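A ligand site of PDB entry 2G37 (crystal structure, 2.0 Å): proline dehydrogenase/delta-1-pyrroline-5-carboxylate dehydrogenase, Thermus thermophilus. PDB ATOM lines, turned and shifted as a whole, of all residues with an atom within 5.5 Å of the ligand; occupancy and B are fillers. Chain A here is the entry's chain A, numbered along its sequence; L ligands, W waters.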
ATOM      1  N   ILE A  79      -2.995  16.515  22.905  1.00  0.00           N
ATOM      2  CA  ILE A  79      -4.315  16.492  23.468  1.00  0.00           C
ATOM      3  C   ILE A  79      -5.234  16.804  22.306  1.00  0.00           C
ATOM      4  O   ILE A  79      -5.129  17.890  21.699  1.00  0.00           O
ATOM      5  CB  ILE A  79      -4.508  17.587  24.524  1.00  0.00           C
ATOM      6  CG1 ILE A  79      -3.532  17.372  25.686  1.00  0.00           C
ATOM      7  CG2 ILE A  79      -6.023  17.657  24.968  1.00  0.00           C
ATOM      8  CD1 ILE A  79      -3.272  18.630  26.493  1.00  0.00           C
ATOM      9  N   LEU A 152     -11.948  17.067  31.401  1.00  0.00           N
ATOM     10  CA  LEU A 152     -13.088  17.968  31.413  1.00  0.00           C
ATOM     11  C   LEU A 152     -12.552  19.392  31.441  1.00  0.00           C
ATOM     12  O   LEU A 152     -12.038  19.830  32.464  1.00  0.00           O
ATOM     13  CB  LEU A 152     -13.993  17.717  32.638  1.00  0.00           C
ATOM     14  CG  LEU A 152     -14.463  16.252  32.870  1.00  0.00           C
ATOM     15  CD1 LEU A 152     -15.432  16.113  34.069  1.00  0.00           C
ATOM     16  CD2 LEU A 152     -15.112  15.649  31.622  1.00  0.00           C
ATOM     17  N   ASP A 153     -12.612  20.093  30.320  1.00  0.00           N
ATOM     18  CA  ASP A 153     -12.207  21.508  30.246  1.00  0.00           C
ATOM     19  C   ASP A 153     -13.124  22.393  31.143  1.00  0.00           C
ATOM     20  O   ASP A 153     -14.350  22.249  31.150  1.00  0.00           O
ATOM     21  CB  ASP A 153     -12.283  22.016  28.790  1.00  0.00           C
ATOM     22  CG  ASP A 153     -11.178  21.438  27.884  1.00  0.00           C
ATOM     23  OD1 ASP A 153     -10.288  20.692  28.384  1.00  0.00           O
ATOM     24  OD2 ASP A 153     -11.221  21.719  26.666  1.00  0.00           O
ATOM     25  N   MET A 154     -12.523  23.325  31.867  1.00  0.00           N
ATOM     26  CA  MET A 154     -13.319  24.160  32.744  1.00  0.00           C
ATOM     27  C   MET A 154     -13.872  25.360  31.971  1.00  0.00           C
ATOM     28  O   MET A 154     -13.132  26.058  31.277  1.00  0.00           O
ATOM     29  CB  MET A 154     -12.542  24.569  34.004  1.00  0.00           C
ATOM     30  CG  MET A 154     -13.495  25.010  35.182  1.00  0.00           C
ATOM     31  SD  MET A 154     -14.675  23.763  35.817  1.00  0.00           S
ATOM     32  CE  MET A 154     -13.850  23.372  37.310  1.00  0.00           C
ATOM     33  N   GLU A 155     -15.175  25.564  32.086  1.00  0.00           N
ATOM     34  CA  GLU A 155     -15.819  26.689  31.437  1.00  0.00           C
ATOM     35  C   GLU A 155     -15.991  27.834  32.395  1.00  0.00           C
ATOM     36  O   GLU A 155     -15.149  27.973  33.323  1.00  0.00           O
ATOM     37  CB  GLU A 155     -17.109  26.277  30.708  1.00  0.00           C
ATOM     38  CG  GLU A 155     -16.752  25.370  29.534  1.00  0.00           C
ATOM     39  CD  GLU A 155     -17.941  24.712  28.922  1.00  0.00           C
ATOM     40  OE1 GLU A 155     -18.524  25.313  27.993  1.00  0.00           O
ATOM     41  OE2 GLU A 155     -18.267  23.581  29.345  1.00  0.00           O
ATOM     42  N   VAL A 181      -9.912  20.645  35.274  1.00  0.00           N
ATOM     43  CA  VAL A 181      -9.119  21.855  35.064  1.00  0.00           C
ATOM     44  C   VAL A 181      -9.532  22.807  36.170  1.00  0.00           C
ATOM     45  O   VAL A 181     -10.710  22.972  36.428  1.00  0.00           O
ATOM     46  CB  VAL A 181      -9.408  22.483  33.640  1.00  0.00           C
ATOM     47  CG1 VAL A 181      -8.587  23.714  33.422  1.00  0.00           C
ATOM     48  CG2 VAL A 181      -9.118  21.470  32.539  1.00  0.00           C
ATOM     49  N   GLN A 183      -8.847  26.906  37.492  1.00  0.00           N
ATOM     50  CA  GLN A 183      -8.406  28.173  36.953  1.00  0.00           C
ATOM     51  C   GLN A 183      -7.972  29.064  38.106  1.00  0.00           C
ATOM     52  O   GLN A 183      -8.739  29.289  39.068  1.00  0.00           O
ATOM     53  CB  GLN A 183      -9.555  28.863  36.233  1.00  0.00           C
ATOM     54  CG  GLN A 183     -10.112  28.090  35.064  1.00  0.00           C
ATOM     55  CD  GLN A 183     -11.594  28.295  34.914  1.00  0.00           C
ATOM     56  OE1 GLN A 183     -12.319  28.368  35.920  1.00  0.00           O
ATOM     57  NE2 GLN A 183     -12.075  28.388  33.678  1.00  0.00           N
ATOM     58  N   TYR A 185      -7.526  32.255  38.321  1.00  0.00           N
ATOM     59  CA  TYR A 185      -8.110  33.578  38.538  1.00  0.00           C
ATOM     60  C   TYR A 185      -9.324  33.568  39.480  1.00  0.00           C
ATOM     61  O   TYR A 185      -9.726  34.613  39.926  1.00  0.00           O
ATOM     62  CB  TYR A 185      -8.442  34.352  37.250  1.00  0.00           C
ATOM     63  CG  TYR A 185      -9.477  33.753  36.293  1.00  0.00           C
ATOM     64  CD1 TYR A 185      -9.722  34.377  35.073  1.00  0.00           C
ATOM     65  CD2 TYR A 185     -10.168  32.575  36.579  1.00  0.00           C
ATOM     66  CE1 TYR A 185     -10.669  33.860  34.177  1.00  0.00           C
ATOM     67  CE2 TYR A 185     -11.102  32.066  35.668  1.00  0.00           C
ATOM     68  CZ  TYR A 185     -11.345  32.710  34.475  1.00  0.00           C
ATOM     69  OH  TYR A 185     -12.241  32.175  33.542  1.00  0.00           O
ATOM     70  N   ARG A 204      -5.252  19.804  35.539  1.00  0.00           N
ATOM     71  CA  ARG A 204      -4.621  20.778  34.638  1.00  0.00           C
ATOM     72  C   ARG A 204      -4.854  22.149  35.263  1.00  0.00           C
ATOM     73  O   ARG A 204      -5.977  22.462  35.600  1.00  0.00           O
ATOM     74  CB  ARG A 204      -5.209  20.762  33.214  1.00  0.00           C
ATOM     75  CG  ARG A 204      -4.698  21.933  32.350  1.00  0.00           C
ATOM     76  CD  ARG A 204      -5.618  22.176  31.097  1.00  0.00           C
ATOM     77  NE  ARG A 204      -5.640  21.005  30.212  1.00  0.00           N
ATOM     78  CZ  ARG A 204      -6.628  20.699  29.372  1.00  0.00           C
ATOM     79  NH1 ARG A 204      -6.525  19.601  28.616  1.00  0.00           N
ATOM     80  NH2 ARG A 204      -7.681  21.489  29.247  1.00  0.00           N
ATOM     81  N   VAL A 206      -4.765  26.131  34.865  1.00  0.00           N
ATOM     82  CA  VAL A 206      -4.745  27.211  33.902  1.00  0.00           C
ATOM     83  C   VAL A 206      -4.959  28.515  34.638  1.00  0.00           C
ATOM     84  O   VAL A 206      -5.371  28.506  35.800  1.00  0.00           O
ATOM     85  CB  VAL A 206      -5.829  27.041  32.809  1.00  0.00           C
ATOM     86  CG1 VAL A 206      -5.656  25.765  32.053  1.00  0.00           C
ATOM     87  CG2 VAL A 206      -7.266  27.119  33.379  1.00  0.00           C
ATOM     88  N   LYS A 207      -4.639  29.635  33.980  1.00  0.00           N
ATOM     89  CA  LYS A 207      -5.007  30.945  34.516  1.00  0.00           C
ATOM     90  C   LYS A 207      -6.520  31.181  34.453  1.00  0.00           C
ATOM     91  O   LYS A 207      -7.111  31.728  35.403  1.00  0.00           O
ATOM     92  CB  LYS A 207      -4.230  32.061  33.809  1.00  0.00           C
ATOM     93  CG  LYS A 207      -2.710  32.097  34.181  1.00  0.00           C
ATOM     94  CD  LYS A 207      -2.022  33.291  33.579  1.00  0.00           C
ATOM     95  CE  LYS A 207      -0.508  33.183  33.762  1.00  0.00           C
ATOM     96  NZ  LYS A 207       0.120  34.407  33.165  1.00  0.00           N
ATOM     97  N   GLY A 208      -7.146  30.789  33.330  1.00  0.00           N
ATOM     98  CA  GLY A 208      -8.568  30.952  33.112  1.00  0.00           C
ATOM     99  C   GLY A 208      -8.824  31.825  31.882  1.00  0.00           C
ATOM    100  O   GLY A 208      -8.088  32.789  31.641  1.00  0.00           O
ATOM    101  N   ALA A 209      -9.828  31.474  31.075  1.00  0.00           N
ATOM    102  CA  ALA A 209     -10.039  32.097  29.772  1.00  0.00           C
ATOM    103  C   ALA A 209     -11.209  33.045  29.683  1.00  0.00           C
ATOM    104  O   ALA A 209     -11.343  33.705  28.661  1.00  0.00           O
ATOM    105  CB  ALA A 209     -10.200  31.026  28.707  1.00  0.00           C
ATOM    106  N   TYR A 210     -12.068  33.104  30.709  1.00  0.00           N
ATOM    107  CA  TYR A 210     -13.341  33.886  30.589  1.00  0.00           C
ATOM    108  C   TYR A 210     -13.280  35.263  31.230  1.00  0.00           C
ATOM    109  O   TYR A 210     -12.372  35.530  31.997  1.00  0.00           O
ATOM    110  CB  TYR A 210     -14.521  33.066  31.142  1.00  0.00           C
ATOM    111  CG  TYR A 210     -14.652  31.763  30.437  1.00  0.00           C
ATOM    112  CD1 TYR A 210     -15.486  31.654  29.291  1.00  0.00           C
ATOM    113  CD2 TYR A 210     -13.921  30.636  30.836  1.00  0.00           C
ATOM    114  CE1 TYR A 210     -15.606  30.440  28.597  1.00  0.00           C
ATOM    115  CE2 TYR A 210     -14.015  29.458  30.154  1.00  0.00           C
ATOM    116  CZ  TYR A 210     -14.864  29.356  29.042  1.00  0.00           C
ATOM    117  OH  TYR A 210     -14.929  28.166  28.378  1.00  0.00           O
ATOM    118  N   LYS A 221      -3.952  41.041  37.218  1.00  0.00           N
ATOM    119  CA  LYS A 221      -3.126  39.984  36.622  1.00  0.00           C
ATOM    120  C   LYS A 221      -1.926  39.494  37.500  1.00  0.00           C
ATOM    121  O   LYS A 221      -1.580  38.326  37.466  1.00  0.00           O
ATOM    122  CB  LYS A 221      -2.628  40.422  35.227  1.00  0.00           C
ATOM    123  CG  LYS A 221      -2.030  39.280  34.395  1.00  0.00           C
ATOM    124  CD  LYS A 221      -3.018  38.111  34.206  1.00  0.00           C
ATOM    125  CE  LYS A 221      -2.399  36.957  33.427  1.00  0.00           C
ATOM    126  NZ  LYS A 221      -2.185  37.375  31.976  1.00  0.00           N
ATOM    127  N   ASP A 225      -1.511  35.487  38.498  1.00  0.00           N
ATOM    128  CA  ASP A 225      -0.228  34.842  38.272  1.00  0.00           C
ATOM    129  C   ASP A 225       0.297  34.325  39.615  1.00  0.00           C
ATOM    130  O   ASP A 225       0.785  33.210  39.671  1.00  0.00           O
ATOM    131  CB  ASP A 225       0.804  35.847  37.742  1.00  0.00           C
ATOM    132  CG  ASP A 225       0.583  36.196  36.266  1.00  0.00           C
ATOM    133  OD1 ASP A 225      -0.316  35.662  35.625  1.00  0.00           O
ATOM    134  OD2 ASP A 225       1.353  37.042  35.742  1.00  0.00           O
ATOM    135  N   TYR A 228      -1.606  31.317  40.470  1.00  0.00           N
ATOM    136  CA  TYR A 228      -1.248  30.204  39.644  1.00  0.00           C
ATOM    137  C   TYR A 228      -0.067  29.449  40.303  1.00  0.00           C
ATOM    138  O   TYR A 228      -0.095  28.213  40.477  1.00  0.00           O
ATOM    139  CB  TYR A 228      -0.901  30.694  38.216  1.00  0.00           C
ATOM    140  CG  TYR A 228      -0.746  29.582  37.231  1.00  0.00           C
ATOM    141  CD1 TYR A 228      -1.775  29.247  36.341  1.00  0.00           C
ATOM    142  CD2 TYR A 228       0.391  28.775  37.250  1.00  0.00           C
ATOM    143  CE1 TYR A 228      -1.612  28.161  35.460  1.00  0.00           C
ATOM    144  CE2 TYR A 228       0.549  27.741  36.391  1.00  0.00           C
ATOM    145  CZ  TYR A 228      -0.458  27.413  35.509  1.00  0.00           C
ATOM    146  OH  TYR A 228      -0.268  26.318  34.674  1.00  0.00           O
ATOM    147  N   ALA A 245      -0.679  24.153  32.246  1.00  0.00           N
ATOM    148  CA  ALA A 245      -1.159  24.627  30.963  1.00  0.00           C
ATOM    149  C   ALA A 245      -1.064  26.135  30.910  1.00  0.00           C
ATOM    150  O   ALA A 245      -1.987  26.867  31.304  1.00  0.00           O
ATOM    151  CB  ALA A 245      -2.557  24.136  30.678  1.00  0.00           C
ATOM    152  N   THR A 246       0.092  26.591  30.451  1.00  0.00           N
ATOM    153  CA  THR A 246       0.452  27.996  30.447  1.00  0.00           C
ATOM    154  C   THR A 246       1.559  28.228  29.426  1.00  0.00           C
ATOM    155  O   THR A 246       2.373  27.330  29.166  1.00  0.00           O
ATOM    156  CB  THR A 246       0.880  28.497  31.891  1.00  0.00           C
ATOM    157  OG1 THR A 246       1.137  29.905  31.856  1.00  0.00           O
ATOM    158  CG2 THR A 246       2.118  27.803  32.418  1.00  0.00           C
ATOM    159  N   HIS A 247       1.554  29.405  28.800  1.00  0.00           N
ATOM    160  CA  HIS A 247       2.625  29.797  27.884  1.00  0.00           C
ATOM    161  C   HIS A 247       3.579  30.795  28.549  1.00  0.00           C
ATOM    162  O   HIS A 247       4.565  31.200  27.933  1.00  0.00           O
ATOM    163  CB  HIS A 247       2.059  30.434  26.595  1.00  0.00           C
ATOM    164  CG  HIS A 247       1.020  29.598  25.910  1.00  0.00           C
ATOM    165  ND1 HIS A 247      -0.291  30.008  25.770  1.00  0.00           N
ATOM    166  CD2 HIS A 247       1.088  28.367  25.354  1.00  0.00           C
ATOM    167  CE1 HIS A 247      -0.980  29.065  25.161  1.00  0.00           C
ATOM    168  NE2 HIS A 247      -0.175  28.054  24.894  1.00  0.00           N
ATOM    169  N   ASP A 248       3.301  31.131  29.801  1.00  0.00           N
ATOM    170  CA  ASP A 248       3.961  32.226  30.516  1.00  0.00           C
ATOM    171  C   ASP A 248       5.396  31.791  30.891  1.00  0.00           C
ATOM    172  O   ASP A 248       5.562  30.871  31.698  1.00  0.00           O
ATOM    173  CB  ASP A 248       3.124  32.556  31.782  1.00  0.00           C
ATOM    174  CG  ASP A 248       3.680  33.739  32.578  1.00  0.00           C
ATOM    175  OD1 ASP A 248       4.903  33.932  32.579  1.00  0.00           O
ATOM    176  OD2 ASP A 248       2.897  34.494  33.187  1.00  0.00           O
ATOM    177  N   PRO A 249       6.426  32.447  30.311  1.00  0.00           N
ATOM    178  CA  PRO A 249       7.796  31.967  30.579  1.00  0.00           C
ATOM    179  C   PRO A 249       8.286  32.241  32.006  1.00  0.00           C
ATOM    180  O   PRO A 249       9.174  31.553  32.477  1.00  0.00           O
ATOM    181  CB  PRO A 249       8.635  32.724  29.564  1.00  0.00           C
ATOM    182  CG  PRO A 249       7.904  33.957  29.317  1.00  0.00           C
ATOM    183  CD  PRO A 249       6.442  33.613  29.402  1.00  0.00           C
ATOM    184  N   GLN A 272       1.746  22.058  29.361  1.00  0.00           N
ATOM    185  CA  GLN A 272       0.905  22.002  28.180  1.00  0.00           C
ATOM    186  C   GLN A 272       0.816  23.360  27.503  1.00  0.00           C
ATOM    187  O   GLN A 272       0.764  24.392  28.170  1.00  0.00           O
ATOM    188  CB  GLN A 272      -0.492  21.457  28.503  1.00  0.00           C
ATOM    189  CG  GLN A 272      -0.531  20.137  29.315  1.00  0.00           C
ATOM    190  CD  GLN A 272      -1.979  19.712  29.597  1.00  0.00           C
ATOM    191  OE1 GLN A 272      -2.884  20.546  29.564  1.00  0.00           O
ATOM    192  NE2 GLN A 272      -2.202  18.426  29.862  1.00  0.00           N
ATOM    193  N   PHE A 273       0.807  23.336  26.175  1.00  0.00           N
ATOM    194  CA  PHE A 273       0.750  24.539  25.363  1.00  0.00           C
ATOM    195  C   PHE A 273      -0.384  24.332  24.363  1.00  0.00           C
ATOM    196  O   PHE A 273      -0.690  23.189  24.010  1.00  0.00           O
ATOM    197  CB  PHE A 273       2.054  24.710  24.551  1.00  0.00           C
ATOM    198  CG  PHE A 273       3.281  24.909  25.388  1.00  0.00           C
ATOM    199  CD1 PHE A 273       3.903  26.147  25.439  1.00  0.00           C
ATOM    200  CD2 PHE A 273       3.810  23.841  26.135  1.00  0.00           C
ATOM    201  CE1 PHE A 273       5.018  26.338  26.232  1.00  0.00           C
ATOM    202  CE2 PHE A 273       4.948  24.014  26.939  1.00  0.00           C
ATOM    203  CZ  PHE A 273       5.553  25.262  26.981  1.00  0.00           C
ATOM    204  N   LEU A 274      -0.972  25.414  23.867  1.00  0.00           N
ATOM    205  CA  LEU A 274      -1.762  25.337  22.635  1.00  0.00           C
ATOM    206  C   LEU A 274      -0.868  24.925  21.449  1.00  0.00           C
ATOM    207  O   LEU A 274       0.303  25.283  21.375  1.00  0.00           O
ATOM    208  CB  LEU A 274      -2.496  26.664  22.347  1.00  0.00           C
ATOM    209  CG  LEU A 274      -3.507  27.083  23.452  1.00  0.00           C
ATOM    210  CD1 LEU A 274      -4.252  28.341  23.050  1.00  0.00           C
ATOM    211  CD2 LEU A 274      -4.469  25.952  23.767  1.00  0.00           C
ATOM    212  N   VAL A 277       1.647  27.322  19.489  1.00  0.00           N
ATOM    213  CA  VAL A 277       2.015  28.423  20.381  1.00  0.00           C
ATOM    214  C   VAL A 277       3.284  28.049  21.164  1.00  0.00           C
ATOM    215  O   VAL A 277       3.313  27.027  21.887  1.00  0.00           O
ATOM    216  CB  VAL A 277       0.862  28.837  21.375  1.00  0.00           C
ATOM    217  CG1 VAL A 277       1.344  29.935  22.319  1.00  0.00           C
ATOM    218  CG2 VAL A 277      -0.358  29.332  20.610  1.00  0.00           C
ATOM    219  N   ARG A 278       4.306  28.884  21.019  1.00  0.00           N
ATOM    220  CA  ARG A 278       5.695  28.623  21.482  1.00  0.00           C
ATOM    221  C   ARG A 278       6.145  27.215  21.108  1.00  0.00           C
ATOM    222  O   ARG A 278       6.544  26.413  21.961  1.00  0.00           O
ATOM    223  CB  ARG A 278       5.809  28.883  22.989  1.00  0.00           C
ATOM    224  CG  ARG A 278       5.233  30.246  23.387  1.00  0.00           C
ATOM    225  CD  ARG A 278       5.621  30.647  24.819  1.00  0.00           C
ATOM    226  NE  ARG A 278       7.078  30.666  24.960  1.00  0.00           N
ATOM    227  CZ  ARG A 278       7.732  30.433  26.091  1.00  0.00           C
ATOM    228  NH1 ARG A 278       9.062  30.494  26.103  1.00  0.00           N
ATOM    229  NH2 ARG A 278       7.069  30.149  27.211  1.00  0.00           N
ATOM    230  N   TYR A 295      -2.147  21.074  22.809  1.00  0.00           N
ATOM    231  CA  TYR A 295      -3.597  20.970  22.743  1.00  0.00           C
ATOM    232  C   TYR A 295      -3.989  21.261  21.275  1.00  0.00           C
ATOM    233  O   TYR A 295      -3.846  22.405  20.815  1.00  0.00           O
ATOM    234  CB  TYR A 295      -4.174  22.053  23.649  1.00  0.00           C
ATOM    235  CG  TYR A 295      -5.677  22.114  23.859  1.00  0.00           C
ATOM    236  CD1 TYR A 295      -6.260  21.548  25.006  1.00  0.00           C
ATOM    237  CD2 TYR A 295      -6.503  22.826  22.976  1.00  0.00           C
ATOM    238  CE1 TYR A 295      -7.643  21.606  25.233  1.00  0.00           C
ATOM    239  CE2 TYR A 295      -7.893  22.903  23.193  1.00  0.00           C
ATOM    240  CZ  TYR A 295      -8.450  22.305  24.331  1.00  0.00           C
ATOM    241  OH  TYR A 295      -9.824  22.398  24.569  1.00  0.00           O
ATOM    242  N   GLU A 312      -5.135  37.305  19.908  1.00  0.00           N
ATOM    243  CA  GLU A 312      -4.528  37.331  21.239  1.00  0.00           C
ATOM    244  C   GLU A 312      -3.062  37.777  21.335  1.00  0.00           C
ATOM    245  O   GLU A 312      -2.567  38.036  22.449  1.00  0.00           O
ATOM    246  CB  GLU A 312      -4.690  35.967  21.926  1.00  0.00           C
ATOM    247  CG  GLU A 312      -3.728  34.878  21.402  1.00  0.00           C
ATOM    248  CD  GLU A 312      -4.018  33.492  21.967  1.00  0.00           C
ATOM    249  OE1 GLU A 312      -5.034  33.332  22.707  1.00  0.00           O
ATOM    250  OE2 GLU A 312      -3.231  32.547  21.647  1.00  0.00           O
ATOM    251  N   ARG A 313      -2.366  37.851  20.194  1.00  0.00           N
ATOM    252  CA  ARG A 313      -0.910  38.069  20.153  1.00  0.00           C
ATOM    253  C   ARG A 313      -0.457  38.563  18.776  1.00  0.00           C
ATOM    254  O   ARG A 313      -0.432  37.772  17.840  1.00  0.00           O
ATOM    255  CB  ARG A 313      -0.181  36.762  20.502  1.00  0.00           C
ATOM    256  CG  ARG A 313       1.322  36.885  20.791  1.00  0.00           C
ATOM    257  CD  ARG A 313       1.599  37.559  22.151  1.00  0.00           C
ATOM    258  NE  ARG A 313       0.708  37.082  23.220  1.00  0.00           N
ATOM    259  CZ  ARG A 313       0.748  37.507  24.478  1.00  0.00           C
ATOM    260  NH1 ARG A 313       1.629  38.419  24.855  1.00  0.00           N
ATOM    261  NH2 ARG A 313      -0.106  37.013  25.373  1.00  0.00           N
HETATM  262  P1  LIG L   1      -0.866  34.884  29.511  1.00  0.00           P
HETATM  263  O1  LIG L   1      -1.841  35.040  28.378  1.00  0.00           O
HETATM  264  O2  LIG L   1      -1.090  35.515  30.858  1.00  0.00           O
HETATM  265  O3  LIG L   1       0.590  35.372  29.043  1.00  0.00           O
HETATM  266  C1  LIG L   1       1.588  35.625  30.047  1.00  0.00           C
HETATM  267  C2  LIG L   1       2.920  35.640  29.321  1.00  0.00           C
HETATM  268  O4  LIG L   1       3.018  34.434  28.565  1.00  0.00           O
HETATM  269  C3  LIG L   1       2.930  36.753  28.297  1.00  0.00           C
HETATM  270  O5  LIG L   1       3.449  37.952  28.860  1.00  0.00           O
HETATM  271  C4  LIG L   1       3.809  36.203  27.198  1.00  0.00           C
HETATM  272  O6  LIG L   1       5.164  36.501  27.532  1.00  0.00           O
HETATM  273  C5  LIG L   1       3.657  34.701  27.317  1.00  0.00           C
HETATM  274  N1  LIG L   1       2.876  34.265  26.137  1.00  0.00           N
HETATM  275  C6  LIG L   1       1.562  34.057  26.038  1.00  0.00           C
HETATM  276  N2  LIG L   1       1.276  33.702  24.759  1.00  0.00           N
HETATM  277  C7  LIG L   1       2.432  33.711  24.063  1.00  0.00           C
HETATM  278  C8  LIG L   1       2.775  33.451  22.736  1.00  0.00           C
HETATM  279  N3  LIG L   1       1.815  33.110  21.860  1.00  0.00           N
HETATM  280  N4  LIG L   1       4.072  33.553  22.346  1.00  0.00           N
HETATM  281  C9  LIG L   1       5.042  33.915  23.214  1.00  0.00           C
HETATM  282  N5  LIG L   1       4.737  34.183  24.493  1.00  0.00           N
HETATM  283  C10 LIG L   1       3.442  34.080  24.940  1.00  0.00           C
HETATM  284  N6  LIG L   1      -8.731  28.022  30.106  1.00  0.00           N
HETATM  285  C11 LIG L   1      -9.915  27.705  30.667  1.00  0.00           C
HETATM  286  O7  LIG L   1     -10.602  28.609  31.165  1.00  0.00           O
HETATM  287  N7  LIG L   1     -10.322  26.428  30.723  1.00  0.00           N
HETATM  288  C12 LIG L   1      -9.547  25.426  30.223  1.00  0.00           C
HETATM  289  O8  LIG L   1      -9.979  24.247  30.294  1.00  0.00           O
HETATM  290  C13 LIG L   1      -8.318  25.707  29.628  1.00  0.00           C
HETATM  291  N8  LIG L   1      -7.514  24.725  29.106  1.00  0.00           N
HETATM  292  C14 LIG L   1      -6.295  25.044  28.547  1.00  0.00           C
HETATM  293  C15 LIG L   1      -5.433  24.057  28.031  1.00  0.00           C
HETATM  294  C16 LIG L   1      -4.192  24.394  27.472  1.00  0.00           C
HETATM  295  C17 LIG L   1      -3.280  23.287  26.925  1.00  0.00           C
HETATM  296  C18 LIG L   1      -3.799  25.735  27.464  1.00  0.00           C
HETATM  297  C19 LIG L   1      -2.497  26.221  26.891  1.00  0.00           C
HETATM  298  C20 LIG L   1      -4.655  26.736  27.965  1.00  0.00           C
HETATM  299  C21 LIG L   1      -5.892  26.372  28.499  1.00  0.00           C
HETATM  300  N9  LIG L   1      -6.734  27.391  29.034  1.00  0.00           N
HETATM  301  C22 LIG L   1      -7.934  27.058  29.575  1.00  0.00           C
HETATM  302  C23 LIG L   1      -6.324  28.786  28.899  1.00  0.00           C
HETATM  303  C24 LIG L   1      -5.751  29.628  30.019  1.00  0.00           C
HETATM  304  O9  LIG L   1      -6.796  29.758  30.978  1.00  0.00           O
HETATM  305  C25 LIG L   1      -5.272  30.995  29.507  1.00  0.00           C
HETATM  306  O10 LIG L   1      -6.377  31.819  29.102  1.00  0.00           O
HETATM  307  C26 LIG L   1      -4.264  30.950  28.334  1.00  0.00           C
HETATM  308  O11 LIG L   1      -3.363  29.841  28.450  1.00  0.00           O
HETATM  309  C27 LIG L   1      -3.357  32.170  28.310  1.00  0.00           C
HETATM  310  O12 LIG L   1      -2.718  32.367  29.586  1.00  0.00           O
HETATM  311  P2  LIG L   1      -1.169  31.990  29.777  1.00  0.00           P
HETATM  312  O13 LIG L   1      -0.857  31.366  31.123  1.00  0.00           O
HETATM  313  O14 LIG L   1      -0.663  31.237  28.582  1.00  0.00           O
HETATM  314  O15 LIG L   1      -0.401  33.362  29.780  1.00  0.00           O
HETATM  315  O   HOH W   1       4.111  31.699  19.501  1.00  0.00           O
HETATM  316  O   HOH W   2      -2.883  29.432  31.734  1.00  0.00           O
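Water W2 lies within hydrogen-bond range of the backbone carbonyl oxygen of Ala 245 (2.8 Å), the backbone NH of Lys 207 (2.9 Å) and an oxygen (O13) of the ligand (2.9 Å). Water W1 lies within hydrogen-bond range of N of Arg 278 (3.2 Å) and N4 of the ligand (3.4 Å).
Merely in contact with the ligand: Asp 248, Val 277, Val 206, Val 181, Leu 274, Asp 153, Ala 245, Tyr 295, Pro 249, Arg 278, Tyr 210, Gln 272 and Phe 273. The nearest printed residue that does not touch the ligand is Tyr 185 (4.6 Å).
OD2 of Asp 248 lies within salt-bridge range of NZ of Lys 207 (2.8 Å). The backbone carbonyl oxygen (O) of Lys 207 sits at hydrogen-bond distance from the backbone NH (N) of Tyr 185 (3.0 Å). The guanidinium group (NH2) of Arg 278 lies within hydrogen-bond range of the backbone carbonyl oxygen (O) of His 247, at 2.8 Å. NH2 of Arg 204 lies within salt-bridge range of OD1 of Asp 153, at 2.9 Å. The side-chain amide oxygen (OE1) of Gln 272 is in hydrogen-bond range of the guanidinium group (NE) of Arg 204 (2.9 Å). OD2 of Asp 153 sits at hydrogen-bond distance from OH of Tyr 295, 2.6 Å away. The backbone NH (N) of Ala 245 sits at hydrogen-bond distance from the side-chain hydroxyl (OH) of Tyr 228 (3.3 Å). The backbone NH of Tyr 210 sits at hydrogen-bond distance from the side-chain hydroxyl of Tyr 185, at 3.0 Å.
The side-chain amino group (NZ) of Lys 221 is in salt-bridge range of an oxygen (O2) of the ligand. OG1 of Thr 246 lies within hydrogen-bond range of O13 of the ligand, at 2.6 Å. An oxygen (O9) of the ligand sits at hydrogen-bond distance from the backbone NH (N) of Gly 208 (2.6 Å). An oxygen (O10) of the ligand sits at hydrogen-bond distance from the backbone carbonyl oxygen (O) of Gly 208, at 3.2 Å. NZ of Lys 207 is in salt-bridge range of O2 of the ligand (2.8 Å). An oxygen (O14) of the ligand sits at hydrogen-bond distance from the backbone NH of His 247 (2.9 Å). A ring nitrogen (ND1) of His 247 is in hydrogen-bond range of an oxygen (O14) of the ligand. The backbone NH of Met 154 is in hydrogen-bond range of an oxygen (O8) of the ligand, at 3.1 Å. A nitrogen (N7) of the ligand is in hydrogen-bond range of the backbone carbonyl oxygen (O) of Met 154, at 2.9 Å. The side-chain amide nitrogen (NE2) of Gln 183 lies within hydrogen-bond range of an oxygen (O7) of the ligand, 2.9 Å away. The backbone NH of Ala 209 is in hydrogen-bond range of an oxygen (O7) of the ligand. The guanidinium group (NH2) of Arg 204 is in hydrogen-bond range of a nitrogen (N8) of the ligand. The guanidinium group (NH2) of Arg 313 lies within salt-bridge range of an oxygen (O1) of the ligand, at 3.99 Å.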
